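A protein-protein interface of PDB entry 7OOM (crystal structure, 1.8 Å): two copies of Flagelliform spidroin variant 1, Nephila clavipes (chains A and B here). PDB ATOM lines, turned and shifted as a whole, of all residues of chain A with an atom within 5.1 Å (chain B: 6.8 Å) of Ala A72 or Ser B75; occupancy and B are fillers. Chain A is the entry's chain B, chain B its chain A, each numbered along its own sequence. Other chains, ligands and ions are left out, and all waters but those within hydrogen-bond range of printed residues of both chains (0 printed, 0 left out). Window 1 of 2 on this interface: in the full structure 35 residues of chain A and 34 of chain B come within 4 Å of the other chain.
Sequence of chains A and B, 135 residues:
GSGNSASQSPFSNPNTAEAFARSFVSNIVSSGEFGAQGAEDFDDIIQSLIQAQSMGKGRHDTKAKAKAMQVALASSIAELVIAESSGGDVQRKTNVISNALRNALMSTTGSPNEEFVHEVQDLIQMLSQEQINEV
OG of Ser B75 lies within hydrogen-bond range of OG of Ser A75 (2.6 Å).
The backbone carbonyl oxygen of Val B71 sits at hydrogen-bond distance from the side-chain hydroxyl of Ser B75 (3.2 Å).
The side-chain hydroxyl (OG) of Ser B75 lies within hydrogen-bond range of the backbone carbonyl oxygen (O) of Ala B72 (2.9 Å).
The backbone carbonyl oxygen of Leu B73 lies within hydrogen-bond range of the side-chain hydroxyl of Ser B76 (2.8 Å).
The backbone carbonyl oxygen (O) of Val A71 lies within hydrogen-bond range of the side-chain hydroxyl (OG) of Ser A75 (3.3 Å).
OG of Ser A75 is in hydrogen-bond range of O of Ala A72.
O of Leu A73 is in hydrogen-bond range of OG of Ser A76 (2.9 Å).
Among the printed residues, pairs that only touch across the chains: Ala A72 with Ser B75, Ser A75 with Ala B72, Met A69 with Ile B45, Ala A68 with Glu B79, Ser A75 with Val B71, Lys A67 with Glu B79, Val A71 with Ser B75, Leu A49 with Leu B49, Ala A72 with Ala B72, Val A71 with Glu B79, Ala A68 with Ser B76, Ala A68 with Leu B80, Ser A76 with Ala B68 and Val A71 with Leu B127.
Of the printed residues of chain B, Ala A72 touches Ala B72 (3.7 Å) and Ser B75 (3.3 Å).
Of the printed residues of chain A, Ser B75 touches Val A71 (3.7 Å), Ala A72 (3.3 Å) and Ser A75 (2.6 Å).
Printed residues of chain B within 4 Å of Met A69: Ile B45 (3.5 Å).
Of the printed residues of chain B, Lys A67 touches Glu B79 (3.6 Å).
Of the printed residues of chain A, Leu B49 touches Leu A49.
Printed residues of chain A within 4 Å of Ala B68: Ser A76.
Of the printed residues of chain B, Ser A76 touches Ala B68.
The nearest printed residue of chain B that does not touch Ala A72 is Ser B76 (4.1 Å).
The nearest printed residue of chain B that does not touch Met A69 is Leu B49 (4.2 Å).
Among the printed residues, no Asp or Glu carboxylate lies within 4 Å of a Lys or Arg side-chain nitrogen of the other chain.
Leu A49 touches its own counterpart, Leu B49.
Ala A68 touches Ser B76, and with the chains exchanged Ser A76 touches Ala B68.
Val A71 touches Ser B75, and with the chains exchanged Ser A75 touches Val B71.
Ala A72 touches its own counterpart, Ala B72.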
ATOM      1  N   LEU A  49      -3.670 -10.695   4.659  1.00  0.00           N
ATOM      2  CA  LEU A  49      -4.315  -9.750   3.710  1.00  0.00           C
ATOM      3  C   LEU A  49      -3.257  -8.733   3.171  1.00  0.00           C
ATOM      4  O   LEU A  49      -3.455  -8.195   2.080  1.00  0.00           O
ATOM      5  CB  LEU A  49      -5.494  -9.093   4.418  1.00  0.00           C
ATOM      6  CG  LEU A  49      -6.873  -9.710   4.210  1.00  0.00           C
ATOM      7  CD1 LEU A  49      -7.358  -9.554   2.762  1.00  0.00           C
ATOM      8  CD2 LEU A  49      -6.897 -11.160   4.633  1.00  0.00           C
ATOM      9  N   LYS A  67      -9.205  -1.099  -4.962  1.00  0.00           N
ATOM     10  CA  LYS A  67     -10.472  -0.967  -4.192  1.00  0.00           C
ATOM     11  C   LYS A  67     -10.901  -2.339  -3.654  1.00  0.00           C
ATOM     12  O   LYS A  67     -11.358  -2.417  -2.502  1.00  0.00           O
ATOM     13  CB  LYS A  67     -11.589  -0.388  -5.081  1.00  0.00           C
ATOM     14  CG  LYS A  67     -11.385   1.085  -5.492  1.00  0.00           C
ATOM     15  CD  LYS A  67     -12.664   1.771  -5.978  1.00  0.00           C
ATOM     16  CE  LYS A  67     -12.506   2.944  -6.931  1.00  0.00           C
ATOM     17  NZ  LYS A  67     -13.378   2.748  -8.120  1.00  0.00           N
ATOM     18  N   ALA A  68     -10.885  -3.388  -4.502  1.00  0.00           N
ATOM     19  CA  ALA A  68     -11.267  -4.769  -4.108  1.00  0.00           C
ATOM     20  C   ALA A  68     -10.408  -5.224  -2.933  1.00  0.00           C
ATOM     21  O   ALA A  68     -10.966  -5.794  -1.985  1.00  0.00           O
ATOM     22  CB  ALA A  68     -11.117  -5.712  -5.284  1.00  0.00           C
ATOM     23  N   MET A  69      -9.097  -4.940  -2.926  1.00  0.00           N
ATOM     24  CA  MET A  69      -8.203  -5.427  -1.845  1.00  0.00           C
ATOM     25  C   MET A  69      -8.385  -4.594  -0.563  1.00  0.00           C
ATOM     26  O   MET A  69      -8.280  -5.164   0.528  1.00  0.00           O
ATOM     27  CB  MET A  69      -6.746  -5.415  -2.332  1.00  0.00           C
ATOM     28  CG  MET A  69      -6.417  -6.530  -3.361  1.00  0.00           C
ATOM     29  SD  MET A  69      -6.834  -8.245  -2.923  1.00  0.00           S
ATOM     30  CE  MET A  69      -6.659  -8.164  -1.169  1.00  0.00           C
ATOM     31  N   GLN A  70      -8.799  -3.336  -0.650  1.00  0.00           N
ATOM     32  CA  GLN A  70      -9.060  -2.472   0.549  1.00  0.00           C
ATOM     33  C   GLN A  70     -10.351  -2.947   1.200  1.00  0.00           C
ATOM     34  O   GLN A  70     -10.385  -3.117   2.449  1.00  0.00           O
ATOM     35  CB  GLN A  70      -9.195  -0.996   0.173  1.00  0.00           C
ATOM     36  CG  GLN A  70      -9.663  -0.125   1.327  1.00  0.00           C
ATOM     37  CD  GLN A  70      -9.849   1.294   0.868  1.00  0.00           C
ATOM     38  OE1 GLN A  70      -9.012   1.829   0.122  1.00  0.00           O
ATOM     39  NE2 GLN A  70     -10.931   1.909   1.318  1.00  0.00           N
ATOM     40  N   VAL A  71     -11.356  -3.230   0.376  1.00  0.00           N
ATOM     41  CA  VAL A  71     -12.625  -3.819   0.880  1.00  0.00           C
ATOM     42  C   VAL A  71     -12.376  -5.189   1.513  1.00  0.00           C
ATOM     43  O   VAL A  71     -12.989  -5.473   2.551  1.00  0.00           O
ATOM     44  CB  VAL A  71     -13.707  -3.800  -0.206  1.00  0.00           C
ATOM     45  CG1 VAL A  71     -14.891  -4.646   0.202  1.00  0.00           C
ATOM     46  CG2 VAL A  71     -14.149  -2.367  -0.500  1.00  0.00           C
ATOM     47  N   ALA A  72     -11.565  -6.055   0.905  1.00  0.00           N
ATOM     48  CA  ALA A  72     -11.263  -7.392   1.462  1.00  0.00           C
ATOM     49  C   ALA A  72     -10.643  -7.235   2.858  1.00  0.00           C
ATOM     50  O   ALA A  72     -11.107  -7.894   3.766  1.00  0.00           O
ATOM     51  CB  ALA A  72     -10.330  -8.164   0.540  1.00  0.00           C
ATOM     52  N   LEU A  73      -9.713  -6.297   3.040  1.00  0.00           N
ATOM     53  CA  LEU A  73      -9.042  -6.025   4.338  1.00  0.00           C
ATOM     54  C   LEU A  73     -10.078  -5.506   5.327  1.00  0.00           C
ATOM     55  O   LEU A  73     -10.169  -6.050   6.447  1.00  0.00           O
ATOM     56  CB  LEU A  73      -7.907  -5.004   4.162  1.00  0.00           C
ATOM     57  CG  LEU A  73      -7.302  -4.541   5.481  1.00  0.00           C
ATOM     58  CD1 LEU A  73      -6.664  -5.703   6.181  1.00  0.00           C
ATOM     59  CD2 LEU A  73      -6.291  -3.399   5.262  1.00  0.00           C
ATOM     60  N   ALA A  74     -10.915  -4.545   4.930  1.00  0.00           N
ATOM     61  CA  ALA A  74     -11.959  -3.979   5.813  1.00  0.00           C
ATOM     62  C   ALA A  74     -12.945  -5.078   6.272  1.00  0.00           C
ATOM     63  O   ALA A  74     -13.311  -5.116   7.459  1.00  0.00           O
ATOM     64  CB  ALA A  74     -12.690  -2.835   5.103  1.00  0.00           C
ATOM     65  N   SER A  75     -13.333  -5.989   5.366  1.00  0.00           N
ATOM     66  CA  SER A  75     -14.355  -7.039   5.623  1.00  0.00           C
ATOM     67  C   SER A  75     -13.762  -8.093   6.556  1.00  0.00           C
ATOM     68  O   SER A  75     -14.505  -8.619   7.437  1.00  0.00           O
ATOM     69  CB  SER A  75     -14.873  -7.663   4.350  1.00  0.00           C
ATOM     70  OG  SER A  75     -13.885  -8.455   3.708  1.00  0.00           O
ATOM     71  N   SER A  76     -12.467  -8.364   6.398  1.00  0.00           N
ATOM     72  CA  SER A  76     -11.772  -9.367   7.234  1.00  0.00           C
ATOM     73  C   SER A  76     -11.726  -8.855   8.674  1.00  0.00           C
ATOM     74  O   SER A  76     -12.013  -9.674   9.606  1.00  0.00           O
ATOM     75  CB  SER A  76     -10.429  -9.759   6.671  1.00  0.00           C
ATOM     76  OG  SER A  76      -9.454  -8.782   6.982  1.00  0.00           O
ATOM     77  N   ILE B  45      -7.338 -11.183  -8.253  1.00  0.00           N
ATOM     78  CA  ILE B  45      -7.855 -10.926  -6.879  1.00  0.00           C
ATOM     79  C   ILE B  45      -8.186 -12.270  -6.229  1.00  0.00           C
ATOM     80  O   ILE B  45      -7.814 -12.516  -5.068  1.00  0.00           O
ATOM     81  CB  ILE B  45      -9.073  -9.983  -6.923  1.00  0.00           C
ATOM     82  CG1 ILE B  45      -8.672  -8.566  -7.335  1.00  0.00           C
ATOM     83  CG2 ILE B  45      -9.780 -10.031  -5.601  1.00  0.00           C
ATOM     84  CD1 ILE B  45      -7.848  -7.815  -6.342  1.00  0.00           C
ATOM     85  N   LEU B  49      -6.311 -14.064  -2.942  1.00  0.00           N
ATOM     86  CA  LEU B  49      -6.994 -14.353  -1.662  1.00  0.00           C
ATOM     87  C   LEU B  49      -6.973 -15.860  -1.392  1.00  0.00           C
ATOM     88  O   LEU B  49      -6.859 -16.236  -0.224  1.00  0.00           O
ATOM     89  CB  LEU B  49      -8.401 -13.783  -1.718  1.00  0.00           C
ATOM     90  CG  LEU B  49      -8.435 -12.293  -1.450  1.00  0.00           C
ATOM     91  CD1 LEU B  49      -9.836 -11.820  -1.619  1.00  0.00           C
ATOM     92  CD2 LEU B  49      -7.881 -11.978  -0.040  1.00  0.00           C
ATOM     93  N   ALA B  68     -13.273 -15.316   8.452  1.00  0.00           N
ATOM     94  CA  ALA B  68     -12.745 -13.983   8.054  1.00  0.00           C
ATOM     95  C   ALA B  68     -12.280 -14.082   6.607  1.00  0.00           C
ATOM     96  O   ALA B  68     -12.525 -13.171   5.829  1.00  0.00           O
ATOM     97  CB  ALA B  68     -11.628 -13.524   8.934  1.00  0.00           C
ATOM     98  N   GLN B  70     -13.306 -16.268   4.298  1.00  0.00           N
ATOM     99  CA  GLN B  70     -14.467 -16.502   3.394  1.00  0.00           C
ATOM    100  C   GLN B  70     -15.156 -15.178   3.092  1.00  0.00           C
ATOM    101  O   GLN B  70     -15.449 -14.870   1.931  1.00  0.00           O
ATOM    102  CB  GLN B  70     -15.466 -17.486   3.967  1.00  0.00           C
ATOM    103  CG  GLN B  70     -16.662 -17.623   3.043  1.00  0.00           C
ATOM    104  CD  GLN B  70     -17.655 -18.664   3.475  1.00  0.00           C
ATOM    105  OE1 GLN B  70     -17.281 -19.804   3.769  1.00  0.00           O
ATOM    106  NE2 GLN B  70     -18.928 -18.281   3.495  1.00  0.00           N
ATOM    107  N   VAL B  71     -15.319 -14.357   4.116  1.00  0.00           N
ATOM    108  CA  VAL B  71     -15.865 -12.989   3.935  1.00  0.00           C
ATOM    109  C   VAL B  71     -14.909 -12.115   3.135  1.00  0.00           C
ATOM    110  O   VAL B  71     -15.374 -11.410   2.293  1.00  0.00           O
ATOM    111  CB  VAL B  71     -16.224 -12.388   5.289  1.00  0.00           C
ATOM    112  CG1 VAL B  71     -16.560 -10.918   5.113  1.00  0.00           C
ATOM    113  CG2 VAL B  71     -17.367 -13.181   5.896  1.00  0.00           C
ATOM    114  N   ALA B  72     -13.602 -12.206   3.313  1.00  0.00           N
ATOM    115  CA  ALA B  72     -12.639 -11.403   2.538  1.00  0.00           C
ATOM    116  C   ALA B  72     -12.809 -11.783   1.053  1.00  0.00           C
ATOM    117  O   ALA B  72     -12.888 -10.886   0.211  1.00  0.00           O
ATOM    118  CB  ALA B  72     -11.216 -11.667   3.029  1.00  0.00           C
ATOM    119  N   LEU B  73     -13.024 -13.066   0.757  1.00  0.00           N
ATOM    120  CA  LEU B  73     -13.122 -13.476  -0.675  1.00  0.00           C
ATOM    121  C   LEU B  73     -14.451 -12.947  -1.234  1.00  0.00           C
ATOM    122  O   LEU B  73     -14.449 -12.417  -2.370  1.00  0.00           O
ATOM    123  CB  LEU B  73     -13.058 -14.989  -0.767  1.00  0.00           C
ATOM    124  CG  LEU B  73     -13.231 -15.578  -2.166  1.00  0.00           C
ATOM    125  CD1 LEU B  73     -12.154 -15.082  -3.112  1.00  0.00           C
ATOM    126  CD2 LEU B  73     -13.220 -17.104  -2.072  1.00  0.00           C
ATOM    127  N   ALA B  74     -15.546 -13.167  -0.504  1.00  0.00           N
ATOM    128  CA  ALA B  74     -16.895 -12.700  -0.914  1.00  0.00           C
ATOM    129  C   ALA B  74     -16.868 -11.193  -1.192  1.00  0.00           C
ATOM    130  O   ALA B  74     -17.451 -10.726  -2.215  1.00  0.00           O
ATOM    131  CB  ALA B  74     -17.900 -13.033   0.141  1.00  0.00           C
ATOM    132  N   SER B  75     -16.277 -10.425  -0.274  1.00  0.00           N
ATOM    133  CA  SER B  75     -16.214  -8.934  -0.325  1.00  0.00           C
ATOM    134  C   SER B  75     -15.370  -8.467  -1.521  1.00  0.00           C
ATOM    135  O   SER B  75     -15.707  -7.442  -2.135  1.00  0.00           O
ATOM    136  CB  SER B  75     -15.714  -8.347   0.994  1.00  0.00           C
ATOM    137  OG  SER B  75     -14.331  -8.634   1.202  1.00  0.00           O
ATOM    138  N   SER B  76     -14.288  -9.172  -1.837  1.00  0.00           N
ATOM    139  CA  SER B  76     -13.379  -8.822  -2.948  1.00  0.00           C
ATOM    140  C   SER B  76     -14.155  -9.003  -4.263  1.00  0.00           C
ATOM    141  O   SER B  76     -14.065  -8.152  -5.193  1.00  0.00           O
ATOM    142  CB  SER B  76     -12.117  -9.628  -2.818  1.00  0.00           C
ATOM    143  OG  SER B  76     -12.268 -10.961  -3.319  1.00  0.00           O
ATOM    144  N   ILE B  77     -14.953 -10.072  -4.357  1.00  0.00           N
ATOM    145  CA  ILE B  77     -15.700 -10.368  -5.601  1.00  0.00           C
ATOM    146  C   ILE B  77     -16.777  -9.288  -5.736  1.00  0.00           C
ATOM    147  O   ILE B  77     -16.955  -8.740  -6.830  1.00  0.00           O
ATOM    148  CB  ILE B  77     -16.259 -11.804  -5.589  1.00  0.00           C
ATOM    149  CG1 ILE B  77     -15.162 -12.866  -5.654  1.00  0.00           C
ATOM    150  CG2 ILE B  77     -17.313 -12.009  -6.672  1.00  0.00           C
ATOM    151  CD1 ILE B  77     -15.664 -14.248  -5.338  1.00  0.00           C
ATOM    152  N   ALA B  78     -17.482  -8.976  -4.647  1.00  0.00           N
ATOM    153  CA  ALA B  78     -18.567  -7.982  -4.653  1.00  0.00           C
ATOM    154  C   ALA B  78     -18.030  -6.610  -5.073  1.00  0.00           C
ATOM    155  O   ALA B  78     -18.733  -5.897  -5.841  1.00  0.00           O
ATOM    156  CB  ALA B  78     -19.185  -7.948  -3.270  1.00  0.00           C
ATOM    157  N   GLU B  79     -16.906  -6.190  -4.504  1.00  0.00           N
ATOM    158  CA  GLU B  79     -16.303  -4.867  -4.783  1.00  0.00           C
ATOM    159  C   GLU B  79     -15.856  -4.789  -6.246  1.00  0.00           C
ATOM    160  O   GLU B  79     -16.084  -3.758  -6.874  1.00  0.00           O
ATOM    161  CB  GLU B  79     -15.137  -4.563  -3.850  1.00  0.00           C
ATOM    162  CG  GLU B  79     -14.503  -3.208  -4.193  1.00  0.00           C
ATOM    163  CD  GLU B  79     -15.480  -2.029  -4.264  1.00  0.00           C
ATOM    164  OE1 GLU B  79     -16.479  -2.041  -3.493  1.00  0.00           O
ATOM    165  OE2 GLU B  79     -15.167  -1.056  -4.989  1.00  0.00           O
ATOM    166  N   LEU B  80     -15.355  -5.876  -6.819  1.00  0.00           N
ATOM    167  CA  LEU B  80     -15.001  -5.892  -8.259  1.00  0.00           C
ATOM    168  C   LEU B  80     -16.221  -5.702  -9.130  1.00  0.00           C
ATOM    169  O   LEU B  80     -16.116  -4.949 -10.121  1.00  0.00           O
ATOM    170  CB  LEU B  80     -14.289  -7.189  -8.624  1.00  0.00           C
ATOM    171  CG  LEU B  80     -12.801  -7.191  -8.394  1.00  0.00           C
ATOM    172  CD1 LEU B  80     -12.271  -8.558  -8.880  1.00  0.00           C
ATOM    173  CD2 LEU B  80     -12.086  -5.995  -9.061  1.00  0.00           C
ATOM    174  N   PHE B 116     -22.676 -18.586   0.453  1.00  0.00           N
ATOM    175  CA  PHE B 116     -21.557 -17.823  -0.148  1.00  0.00           C
ATOM    176  C   PHE B 116     -22.128 -16.871  -1.202  1.00  0.00           C
ATOM    177  O   PHE B 116     -21.746 -15.701  -1.249  1.00  0.00           O
ATOM    178  CB  PHE B 116     -20.510 -18.746  -0.746  1.00  0.00           C
ATOM    179  CG  PHE B 116     -19.289 -17.999  -1.190  1.00  0.00           C
ATOM    180  CD1 PHE B 116     -18.428 -17.413  -0.268  1.00  0.00           C
ATOM    181  CD2 PHE B 116     -19.043 -17.790  -2.536  1.00  0.00           C
ATOM    182  CE1 PHE B 116     -17.358 -16.648  -0.700  1.00  0.00           C
ATOM    183  CE2 PHE B 116     -17.953 -17.042  -2.946  1.00  0.00           C
ATOM    184  CZ  PHE B 116     -17.118 -16.475  -2.030  1.00  0.00           C
ATOM    185  N   GLU B 119     -24.002 -14.003   0.442  1.00  0.00           N
ATOM    186  CA  GLU B 119     -23.045 -13.049   1.061  1.00  0.00           C
ATOM    187  C   GLU B 119     -22.577 -12.055  -0.006  1.00  0.00           C
ATOM    188  O   GLU B 119     -22.496 -10.858   0.280  1.00  0.00           O
ATOM    189  CB  GLU B 119     -21.797 -13.762   1.609  1.00  0.00           C
ATOM    190  CG  GLU B 119     -22.013 -14.477   2.912  1.00  0.00           C
ATOM    191  CD  GLU B 119     -20.889 -15.428   3.335  1.00  0.00           C
ATOM    192  OE1 GLU B 119     -21.107 -16.227   4.266  1.00  0.00           O
ATOM    193  OE2 GLU B 119     -19.824 -15.384   2.699  1.00  0.00           O
ATOM    194  N   VAL B 120     -22.180 -12.565  -1.170  1.00  0.00           N
ATOM    195  CA  VAL B 120     -21.668 -11.746  -2.293  1.00  0.00           C
ATOM    196  C   VAL B 120     -22.782 -10.786  -2.724  1.00  0.00           C
ATOM    197  O   VAL B 120     -22.496  -9.625  -2.870  1.00  0.00           O
ATOM    198  CB  VAL B 120     -21.211 -12.607  -3.475  1.00  0.00           C
ATOM    199  CG1 VAL B 120     -20.956 -11.758  -4.706  1.00  0.00           C
ATOM    200  CG2 VAL B 120     -19.992 -13.450  -3.117  1.00  0.00           C
ATOM    201  N   LEU B 123     -23.332  -8.166  -0.078  1.00  0.00           N
ATOM    202  CA  LEU B 123     -22.157  -7.252  -0.091  1.00  0.00           C
ATOM    203  C   LEU B 123     -22.221  -6.299  -1.293  1.00  0.00           C
ATOM    204  O   LEU B 123     -21.953  -5.076  -1.101  1.00  0.00           O
ATOM    205  CB  LEU B 123     -20.865  -8.084  -0.043  1.00  0.00           C
ATOM    206  CG  LEU B 123     -20.529  -8.696   1.321  1.00  0.00           C
ATOM    207  CD1 LEU B 123     -19.446  -9.765   1.198  1.00  0.00           C
ATOM    208  CD2 LEU B 123     -20.094  -7.637   2.319  1.00  0.00           C
ATOM    209  N   LEU B 127     -22.251  -2.356  -0.749  1.00  0.00           N
ATOM    210  CA  LEU B 127     -21.078  -1.587  -1.262  1.00  0.00           C
ATOM    211  C   LEU B 127     -21.498  -0.598  -2.351  1.00  0.00           C
ATOM    212  O   LEU B 127     -20.810   0.408  -2.509  1.00  0.00           O
ATOM    213  CB  LEU B 127     -20.001  -2.521  -1.810  1.00  0.00           C
ATOM    214  CG  LEU B 127     -19.252  -3.347  -0.776  1.00  0.00           C
ATOM    215  CD1 LEU B 127     -18.524  -4.488  -1.471  1.00  0.00           C
ATOM    216  CD2 LEU B 127     -18.265  -2.507   0.035  1.00  0.00           C
